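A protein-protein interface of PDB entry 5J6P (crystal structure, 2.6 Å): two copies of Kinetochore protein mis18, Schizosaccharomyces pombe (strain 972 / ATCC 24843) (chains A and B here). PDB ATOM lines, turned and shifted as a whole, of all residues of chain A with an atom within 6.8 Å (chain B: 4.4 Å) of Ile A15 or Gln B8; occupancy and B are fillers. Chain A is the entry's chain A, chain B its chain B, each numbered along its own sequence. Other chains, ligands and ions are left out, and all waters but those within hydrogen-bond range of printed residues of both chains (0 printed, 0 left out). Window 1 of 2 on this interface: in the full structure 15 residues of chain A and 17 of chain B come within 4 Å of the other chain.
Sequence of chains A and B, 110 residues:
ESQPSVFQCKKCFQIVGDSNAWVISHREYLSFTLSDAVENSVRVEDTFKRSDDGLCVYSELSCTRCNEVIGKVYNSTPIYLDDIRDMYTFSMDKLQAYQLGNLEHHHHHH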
ATOM      1  N   VAL A   6     -12.873  -9.306 -12.953  1.00  0.00           N
ATOM      2  CA  VAL A   6     -13.308  -9.058 -14.311  1.00  0.00           C
ATOM      3  C   VAL A   6     -13.957  -7.653 -14.270  1.00  0.00           C
ATOM      4  O   VAL A   6     -14.386  -7.174 -13.191  1.00  0.00           O
ATOM      5  CB  VAL A   6     -14.261 -10.199 -14.698  1.00  0.00           C
ATOM      6  CG1 VAL A   6     -15.538  -9.718 -15.378  1.00  0.00           C
ATOM      7  CG2 VAL A   6     -13.530 -11.236 -15.530  1.00  0.00           C
ATOM      8  N   PHE A   7     -13.999  -6.985 -15.418  1.00  0.00           N
ATOM      9  CA  PHE A   7     -14.510  -5.605 -15.505  1.00  0.00           C
ATOM     10  C   PHE A   7     -15.581  -5.472 -16.594  1.00  0.00           C
ATOM     11  O   PHE A   7     -15.394  -5.977 -17.703  1.00  0.00           O
ATOM     12  CB  PHE A   7     -13.363  -4.650 -15.857  1.00  0.00           C
ATOM     13  CG  PHE A   7     -12.214  -4.676 -14.884  1.00  0.00           C
ATOM     14  CD1 PHE A   7     -12.363  -4.144 -13.601  1.00  0.00           C
ATOM     15  CD2 PHE A   7     -10.973  -5.228 -15.249  1.00  0.00           C
ATOM     16  CE1 PHE A   7     -11.320  -4.157 -12.691  1.00  0.00           C
ATOM     17  CE2 PHE A   7      -9.921  -5.246 -14.340  1.00  0.00           C
ATOM     18  CZ  PHE A   7     -10.095  -4.705 -13.061  1.00  0.00           C
ATOM     19  N   GLN A   8     -16.653  -4.728 -16.296  1.00  0.00           N
ATOM     20  CA  GLN A   8     -17.798  -4.538 -17.204  1.00  0.00           C
ATOM     21  C   GLN A   8     -18.259  -3.061 -17.306  1.00  0.00           C
ATOM     22  O   GLN A   8     -18.136  -2.282 -16.365  1.00  0.00           O
ATOM     23  CB  GLN A   8     -19.020  -5.355 -16.729  1.00  0.00           C
ATOM     24  CG  GLN A   8     -18.755  -6.615 -15.903  1.00  0.00           C
ATOM     25  CD  GLN A   8     -19.990  -7.109 -15.155  1.00  0.00           C
ATOM     26  OE1 GLN A   8     -20.865  -7.720 -15.751  1.00  0.00           O
ATOM     27  NE2 GLN A   8     -20.046  -6.872 -13.837  1.00  0.00           N
ATOM     28  N   CYS A   9     -18.877  -2.727 -18.435  1.00  0.00           N
ATOM     29  CA  CYS A   9     -19.483  -1.413 -18.624  1.00  0.00           C
ATOM     30  C   CYS A   9     -20.553  -1.518 -17.529  1.00  0.00           C
ATOM     31  O   CYS A   9     -21.138  -2.578 -17.313  1.00  0.00           O
ATOM     32  CB  CYS A   9     -19.746  -1.152 -20.109  1.00  0.00           C
ATOM     33  SG  CYS A   9     -20.862   0.231 -20.440  1.00  0.00           S
ATOM     34  N   CYS A  12     -24.425  -1.778 -19.750  1.00  0.00           N
ATOM     35  CA  CYS A  12     -24.886  -3.018 -20.332  1.00  0.00           C
ATOM     36  C   CYS A  12     -24.294  -4.297 -19.712  1.00  0.00           C
ATOM     37  O   CYS A  12     -24.812  -5.396 -19.910  1.00  0.00           O
ATOM     38  CB  CYS A  12     -24.505  -3.101 -21.818  1.00  0.00           C
ATOM     39  SG  CYS A  12     -22.740  -2.895 -22.148  1.00  0.00           S
ATOM     40  N   PHE A  13     -23.210  -4.135 -18.964  1.00  0.00           N
ATOM     41  CA  PHE A  13     -22.512  -5.263 -18.354  1.00  0.00           C
ATOM     42  C   PHE A  13     -21.588  -6.137 -19.211  1.00  0.00           C
ATOM     43  O   PHE A  13     -21.219  -7.240 -18.821  1.00  0.00           O
ATOM     44  CB  PHE A  13     -23.572  -6.083 -17.635  1.00  0.00           C
ATOM     45  CG  PHE A  13     -24.427  -5.217 -16.781  1.00  0.00           C
ATOM     46  CD1 PHE A  13     -23.872  -4.555 -15.682  1.00  0.00           C
ATOM     47  CD2 PHE A  13     -25.749  -5.011 -17.070  1.00  0.00           C
ATOM     48  CE1 PHE A  13     -24.640  -3.727 -14.893  1.00  0.00           C
ATOM     49  CE2 PHE A  13     -26.527  -4.153 -16.281  1.00  0.00           C
ATOM     50  CZ  PHE A  13     -25.973  -3.501 -15.206  1.00  0.00           C
ATOM     51  N   GLN A  14     -21.191  -5.603 -20.361  1.00  0.00           N
ATOM     52  CA  GLN A  14     -20.303  -6.289 -21.255  1.00  0.00           C
ATOM     53  C   GLN A  14     -18.946  -6.251 -20.647  1.00  0.00           C
ATOM     54  O   GLN A  14     -18.476  -5.192 -20.269  1.00  0.00           O
ATOM     55  CB  GLN A  14     -20.256  -5.620 -22.617  1.00  0.00           C
ATOM     56  CG  GLN A  14     -19.448  -6.401 -23.632  1.00  0.00           C
ATOM     57  CD  GLN A  14     -19.674  -5.925 -25.045  1.00  0.00           C
ATOM     58  OE1 GLN A  14     -19.346  -4.797 -25.381  1.00  0.00           O
ATOM     59  NE2 GLN A  14     -20.250  -6.779 -25.881  1.00  0.00           N
ATOM     60  N   ILE A  15     -18.346  -7.439 -20.535  1.00  0.00           N
ATOM     61  CA  ILE A  15     -17.013  -7.619 -19.997  1.00  0.00           C
ATOM     62  C   ILE A  15     -15.991  -7.060 -20.994  1.00  0.00           C
ATOM     63  O   ILE A  15     -16.051  -7.364 -22.198  1.00  0.00           O
ATOM     64  CB  ILE A  15     -16.745  -9.085 -19.671  1.00  0.00           C
ATOM     65  CG1 ILE A  15     -17.566  -9.492 -18.447  1.00  0.00           C
ATOM     66  CG2 ILE A  15     -15.258  -9.339 -19.405  1.00  0.00           C
ATOM     67  CD1 ILE A  15     -17.630 -10.999 -18.183  1.00  0.00           C
ATOM     68  N   VAL A  16     -15.081  -6.222 -20.484  1.00  0.00           N
ATOM     69  CA  VAL A  16     -14.063  -5.559 -21.328  1.00  0.00           C
ATOM     70  C   VAL A  16     -12.640  -6.078 -21.098  1.00  0.00           C
ATOM     71  O   VAL A  16     -11.780  -5.920 -21.968  1.00  0.00           O
ATOM     72  CB  VAL A  16     -14.132  -4.012 -21.223  1.00  0.00           C
ATOM     73  CG1 VAL A  16     -15.521  -3.516 -21.583  1.00  0.00           C
ATOM     74  CG2 VAL A  16     -13.748  -3.497 -19.848  1.00  0.00           C
ATOM     75  N   GLY A  17     -12.417  -6.714 -19.948  1.00  0.00           N
ATOM     76  CA  GLY A  17     -11.221  -7.515 -19.666  1.00  0.00           C
ATOM     77  C   GLY A  17     -11.080  -7.717 -18.162  1.00  0.00           C
ATOM     78  O   GLY A  17     -12.058  -7.531 -17.417  1.00  0.00           O
ATOM     79  N   ASP A  18      -9.863  -8.039 -17.701  1.00  0.00           N
ATOM     80  CA  ASP A  18      -9.658  -8.453 -16.294  1.00  0.00           C
ATOM     81  C   ASP A  18      -8.366  -8.003 -15.647  1.00  0.00           C
ATOM     82  O   ASP A  18      -7.463  -7.520 -16.307  1.00  0.00           O
ATOM     83  CB  ASP A  18      -9.732  -9.983 -16.211  1.00  0.00           C
ATOM     84  CG  ASP A  18      -8.819 -10.680 -17.213  1.00  0.00           C
ATOM     85  OD1 ASP A  18      -7.573 -10.524 -17.134  1.00  0.00           O
ATOM     86  OD2 ASP A  18      -9.359 -11.405 -18.074  1.00  0.00           O
ATOM     87  N   VAL A  38     -10.827  -7.218 -24.520  1.00  0.00           N
ATOM     88  CA  VAL A  38     -11.584  -8.034 -25.432  1.00  0.00           C
ATOM     89  C   VAL A  38     -11.874  -7.229 -26.695  1.00  0.00           C
ATOM     90  O   VAL A  38     -12.620  -6.254 -26.640  1.00  0.00           O
ATOM     91  CB  VAL A  38     -12.877  -8.524 -24.748  1.00  0.00           C
ATOM     92  CG1 VAL A  38     -13.626  -9.468 -25.672  1.00  0.00           C
ATOM     93  CG2 VAL A  38     -12.586  -9.174 -23.397  1.00  0.00           C
ATOM     94  N   SER A  41     -15.477  -6.265 -27.666  1.00  0.00           N
ATOM     95  CA  SER A  41     -16.278  -5.511 -26.706  1.00  0.00           C
ATOM     96  C   SER A  41     -15.904  -4.006 -26.561  1.00  0.00           C
ATOM     97  O   SER A  41     -16.509  -3.280 -25.790  1.00  0.00           O
ATOM     98  CB  SER A  41     -16.212  -6.225 -25.361  1.00  0.00           C
ATOM     99  OG  SER A  41     -14.909  -6.112 -24.853  1.00  0.00           O
ATOM    100  N   VAL A  42     -14.970  -3.522 -27.364  1.00  0.00           N
ATOM    101  CA  VAL A  42     -14.358  -2.215 -27.193  1.00  0.00           C
ATOM    102  C   VAL A  42     -13.978  -1.596 -28.546  1.00  0.00           C
ATOM    103  O   VAL A  42     -13.638  -2.335 -29.490  1.00  0.00           O
ATOM    104  CB  VAL A  42     -13.171  -2.432 -26.294  1.00  0.00           C
ATOM    105  CG1 VAL A  42     -11.918  -1.787 -26.806  1.00  0.00           C
ATOM    106  CG2 VAL A  42     -13.529  -1.989 -24.895  1.00  0.00           C
ATOM    107  N   VAL B   6     -15.792 -16.864 -16.048  1.00  0.00           N
ATOM    108  CA  VAL B   6     -16.919 -16.173 -15.417  1.00  0.00           C
ATOM    109  C   VAL B   6     -18.138 -16.378 -16.282  1.00  0.00           C
ATOM    110  O   VAL B   6     -18.008 -16.516 -17.503  1.00  0.00           O
ATOM    111  CB  VAL B   6     -16.611 -14.681 -15.277  1.00  0.00           C
ATOM    112  CG1 VAL B   6     -17.867 -13.841 -15.159  1.00  0.00           C
ATOM    113  CG2 VAL B   6     -15.757 -14.462 -14.044  1.00  0.00           C
ATOM    114  N   PHE B   7     -19.315 -16.394 -15.654  1.00  0.00           N
ATOM    115  CA  PHE B   7     -20.552 -16.770 -16.348  1.00  0.00           C
ATOM    116  C   PHE B   7     -21.565 -15.675 -16.352  1.00  0.00           C
ATOM    117  O   PHE B   7     -21.845 -15.085 -15.293  1.00  0.00           O
ATOM    118  CB  PHE B   7     -21.181 -18.015 -15.689  1.00  0.00           C
ATOM    119  CG  PHE B   7     -20.262 -19.184 -15.668  1.00  0.00           C
ATOM    120  CD1 PHE B   7     -19.913 -19.798 -16.851  1.00  0.00           C
ATOM    121  CD2 PHE B   7     -19.671 -19.609 -14.490  1.00  0.00           C
ATOM    122  CE1 PHE B   7     -19.016 -20.842 -16.859  1.00  0.00           C
ATOM    123  CE2 PHE B   7     -18.784 -20.664 -14.494  1.00  0.00           C
ATOM    124  CZ  PHE B   7     -18.460 -21.277 -15.675  1.00  0.00           C
ATOM    125  N   GLN B   8     -22.173 -15.461 -17.516  1.00  0.00           N
ATOM    126  CA  GLN B   8     -23.219 -14.449 -17.670  1.00  0.00           C
ATOM    127  C   GLN B   8     -24.448 -14.874 -18.454  1.00  0.00           C
ATOM    128  O   GLN B   8     -24.343 -15.624 -19.404  1.00  0.00           O
ATOM    129  CB  GLN B   8     -22.670 -13.275 -18.452  1.00  0.00           C
ATOM    130  CG  GLN B   8     -21.313 -12.722 -18.068  1.00  0.00           C
ATOM    131  CD  GLN B   8     -20.807 -11.840 -19.184  1.00  0.00           C
ATOM    132  OE1 GLN B   8     -20.887 -10.586 -19.131  1.00  0.00           O
ATOM    133  NE2 GLN B   8     -20.388 -12.494 -20.257  1.00  0.00           N
ATOM    134  N   CYS B   9     -25.602 -14.317 -18.105  1.00  0.00           N
ATOM    135  CA  CYS B   9     -26.810 -14.517 -18.900  1.00  0.00           C
ATOM    136  C   CYS B   9     -26.642 -13.907 -20.295  1.00  0.00           C
ATOM    137  O   CYS B   9     -26.459 -12.698 -20.436  1.00  0.00           O
ATOM    138  CB  CYS B   9     -28.023 -13.905 -18.198  1.00  0.00           C
ATOM    139  SG  CYS B   9     -29.371 -13.438 -19.309  1.00  0.00           S
ATOM    140  N   LYS B  10     -26.703 -14.755 -21.318  1.00  0.00           N
ATOM    141  CA  LYS B  10     -26.528 -14.337 -22.712  1.00  0.00           C
ATOM    142  C   LYS B  10     -27.293 -13.091 -23.100  1.00  0.00           C
ATOM    143  O   LYS B  10     -26.882 -12.360 -24.027  1.00  0.00           O
ATOM    144  CB  LYS B  10     -26.967 -15.432 -23.660  1.00  0.00           C
ATOM    145  CG  LYS B  10     -25.957 -16.569 -23.827  1.00  0.00           C
ATOM    146  CD  LYS B  10     -25.858 -16.972 -25.297  1.00  0.00           C
ATOM    147  CE  LYS B  10     -25.725 -18.466 -25.537  1.00  0.00           C
ATOM    148  NZ  LYS B  10     -26.505 -18.794 -26.766  1.00  0.00           N
ATOM    149  N   PHE B  13     -26.177 -10.085 -19.947  1.00  0.00           N
ATOM    150  CA  PHE B  13     -24.766 -10.075 -19.498  1.00  0.00           C
ATOM    151  C   PHE B  13     -24.568  -9.930 -17.980  1.00  0.00           C
ATOM    152  O   PHE B  13     -23.469  -9.645 -17.506  1.00  0.00           O
ATOM    153  CB  PHE B  13     -23.936  -9.023 -20.238  1.00  0.00           C
ATOM    154  CG  PHE B  13     -23.633  -9.328 -21.684  1.00  0.00           C
ATOM    155  CD1 PHE B  13     -23.922 -10.543 -22.288  1.00  0.00           C
ATOM    156  CD2 PHE B  13     -22.969  -8.366 -22.435  1.00  0.00           C
ATOM    157  CE1 PHE B  13     -23.602 -10.780 -23.606  1.00  0.00           C
ATOM    158  CE2 PHE B  13     -22.632  -8.602 -23.748  1.00  0.00           C
ATOM    159  CZ  PHE B  13     -22.966  -9.818 -24.339  1.00  0.00           C
ATOM    160  N   GLN B  14     -25.609 -10.142 -17.202  1.00  0.00           N
ATOM    161  CA  GLN B  14     -25.412 -10.193 -15.786  1.00  0.00           C
ATOM    162  C   GLN B  14     -24.544 -11.385 -15.425  1.00  0.00           C
ATOM    163  O   GLN B  14     -24.796 -12.502 -15.869  1.00  0.00           O
ATOM    164  CB  GLN B  14     -26.744 -10.303 -15.054  1.00  0.00           C
ATOM    165  CG  GLN B  14     -26.527 -10.327 -13.555  1.00  0.00           C
ATOM    166  CD  GLN B  14     -27.797 -10.238 -12.753  1.00  0.00           C
ATOM    167  OE1 GLN B  14     -28.878 -10.768 -13.131  1.00  0.00           O
ATOM    168  NE2 GLN B  14     -27.672  -9.611 -11.605  1.00  0.00           N
ATOM    169  N   ILE B  15     -23.538 -11.150 -14.599  1.00  0.00           N
ATOM    170  CA  ILE B  15     -22.694 -12.238 -14.132  1.00  0.00           C
ATOM    171  C   ILE B  15     -23.449 -12.964 -13.047  1.00  0.00           C
ATOM    172  O   ILE B  15     -23.875 -12.329 -12.098  1.00  0.00           O
ATOM    173  CB  ILE B  15     -21.362 -11.741 -13.566  1.00  0.00           C
ATOM    174  CG1 ILE B  15     -20.472 -11.300 -14.721  1.00  0.00           C
ATOM    175  CG2 ILE B  15     -20.668 -12.819 -12.748  1.00  0.00           C
ATOM    176  CD1 ILE B  15     -19.352 -10.368 -14.304  1.00  0.00           C
ATOM    177  N   LYS B  94     -28.048 -20.852 -22.498  1.00  0.00           N
ATOM    178  CA  LYS B  94     -28.539 -19.613 -21.952  1.00  0.00           C
ATOM    179  C   LYS B  94     -27.472 -18.839 -21.220  1.00  0.00           C
ATOM    180  O   LYS B  94     -27.752 -17.779 -20.729  1.00  0.00           O
ATOM    181  CB  LYS B  94     -29.679 -19.958 -20.983  1.00  0.00           C
ATOM    182  CG  LYS B  94     -30.931 -20.545 -21.652  1.00  0.00           C
ATOM    183  CD  LYS B  94     -31.759 -19.407 -22.198  1.00  0.00           C
ATOM    184  CE  LYS B  94     -33.048 -19.831 -22.848  1.00  0.00           C
ATOM    185  NZ  LYS B  94     -33.784 -18.583 -23.185  1.00  0.00           N
ATOM    186  N   LEU B  95     -26.262 -19.367 -21.125  1.00  0.00           N
ATOM    187  CA  LEU B  95     -25.176 -18.716 -20.390  1.00  0.00           C
ATOM    188  C   LEU B  95     -24.089 -18.396 -21.381  1.00  0.00           C
ATOM    189  O   LEU B  95     -24.200 -18.753 -22.562  1.00  0.00           O
ATOM    190  CB  LEU B  95     -24.600 -19.613 -19.285  1.00  0.00           C
ATOM    191  CG  LEU B  95     -25.295 -19.667 -17.939  1.00  0.00           C
ATOM    192  CD1 LEU B  95     -25.017 -18.437 -17.130  1.00  0.00           C
ATOM    193  CD2 LEU B  95     -26.792 -19.838 -18.099  1.00  0.00           C
ATOM    194  N   GLN B  96     -23.052 -17.713 -20.887  1.00  0.00           N
ATOM    195  CA  GLN B  96     -21.876 -17.354 -21.672  1.00  0.00           C
ATOM    196  C   GLN B  96     -20.665 -17.412 -20.768  1.00  0.00           C
ATOM    197  O   GLN B  96     -20.755 -17.098 -19.582  1.00  0.00           O
ATOM    198  CB  GLN B  96     -22.038 -15.943 -22.173  1.00  0.00           C
ATOM    199  CG  GLN B  96     -21.807 -15.772 -23.639  1.00  0.00           C
ATOM    200  CD  GLN B  96     -21.946 -14.321 -24.010  1.00  0.00           C
ATOM    201  OE1 GLN B  96     -21.515 -13.450 -23.264  1.00  0.00           O
ATOM    202  NE2 GLN B  96     -22.562 -14.044 -25.156  1.00  0.00           N
ATOM    203  N   TYR B  98     -16.579 -16.413 -20.016  1.00  0.00           N
ATOM    204  CA  TYR B  98     -15.467 -15.577 -20.299  1.00  0.00           C
ATOM    205  C   TYR B  98     -14.325 -16.135 -19.474  1.00  0.00           C
ATOM    206  O   TYR B  98     -14.344 -16.051 -18.211  1.00  0.00           O
ATOM    207  CB  TYR B  98     -15.766 -14.110 -19.947  1.00  0.00           C
ATOM    208  CG  TYR B  98     -14.503 -13.290 -19.943  1.00  0.00           C
ATOM    209  CD1 TYR B  98     -13.889 -12.910 -21.156  1.00  0.00           C
ATOM    210  CD2 TYR B  98     -13.881 -12.946 -18.742  1.00  0.00           C
ATOM    211  CE1 TYR B  98     -12.690 -12.211 -21.157  1.00  0.00           C
ATOM    212  CE2 TYR B  98     -12.698 -12.234 -18.736  1.00  0.00           C
ATOM    213  CZ  TYR B  98     -12.106 -11.884 -19.933  1.00  0.00           C
ATOM    214  OH  TYR B  98     -10.927 -11.212 -19.901  1.00  0.00           O
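O of Phe A13 lies close to OE1 of Gln B8 (3.4 Å). OH of Tyr B98 sits at hydrogen-bond distance from OD2 of Asp A18 (2.4 Å).
The backbone carbonyl oxygen (O) of Phe B13 sits close to the side-chain amide oxygen (OE1) of Gln B8 (3.2 Å). The backbone NH of Phe A7 sits at hydrogen-bond distance from the backbone carbonyl oxygen of Gly A17 (2.8 Å). The backbone NH of Val A38 lies within hydrogen-bond range of the backbone carbonyl oxygen of Val A16, 3.0 Å away. The backbone NH (N) of Gln B96 sits at hydrogen-bond distance from the backbone carbonyl oxygen (O) of Gln B8, 2.9 Å away. SG of Cys A12 sits close to N of Gln A14, at 3.6 Å. The backbone carbonyl oxygen (O) of Ser A41 sits close to the side-chain amide oxygen (OE1) of Gln A14 (3.2 Å).
Tyr B98 touches Val A6 (CE2 to CG2, 3.5 Å). OE1 of Gln A8 touches O of Phe B13, at 3.7 Å. OE1 of Gln A8 touches CD1 of Ile B15 (3.4 Å). Phe B13 touches Cys A12. CB of Phe B13 touches O of Phe A13, at 3.5 Å. CD2 of Phe B13 touches CA of Gln A14, at 3.6 Å. OE1 of Gln B8 touches CD1 of Ile A15, 3.4 Å away. Ile A15 touches Tyr B98 (CG2 to CD2, 3.9 Å). Gly A17 touches Tyr B98. Val A38 touches Tyr B98 (CG2 to CE1, 3.8 Å).
Printed residues of chain B within 4 Å of Cys A12: Phe B13 (3.7 Å). Of chain B, only Gln B8 and Tyr B98 come within 4 Å of Ile A15. Of the printed residues of chain B, Asp A18 touches Tyr B98 (2.4 Å). Phe B7 touches none of the printed residues of chain A. Of chain A, only Phe A13 (3.4 Å) and Ile A15 (3.4 Å) come within 4 Å of Gln B8. The nearest residue of chain B that does not touch Ile A15 is Val B6 (4.2 Å).
Printed residues of chain B that touch a printed residue of chain A: Gln B8, Phe B13, Ile B15 and Tyr B98. Hydrophobic or aromatic side chains of chain B that line the printed part of chain A: Phe B13, Ile B15 and Tyr B98.
Gln A8 touches Phe B13, and with the chains exchanged Phe A13 touches Gln B8. Gln A8 touches Ile B15, and with the chains exchanged Ile A15 touches Gln B8. Phe B13 touches its own counterpart, Phe A13. Gln A14 touches Phe B13, but with the chains exchanged Phe A13 does not touch Gln B14 (4.6 Å). Positions printed for both chains: 6, 7, 8, 9, 13, 14 and 15. Of the 12 pairs that touch across the chains among the printed residues, 5 have their exchanged pair printed and touching as well.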
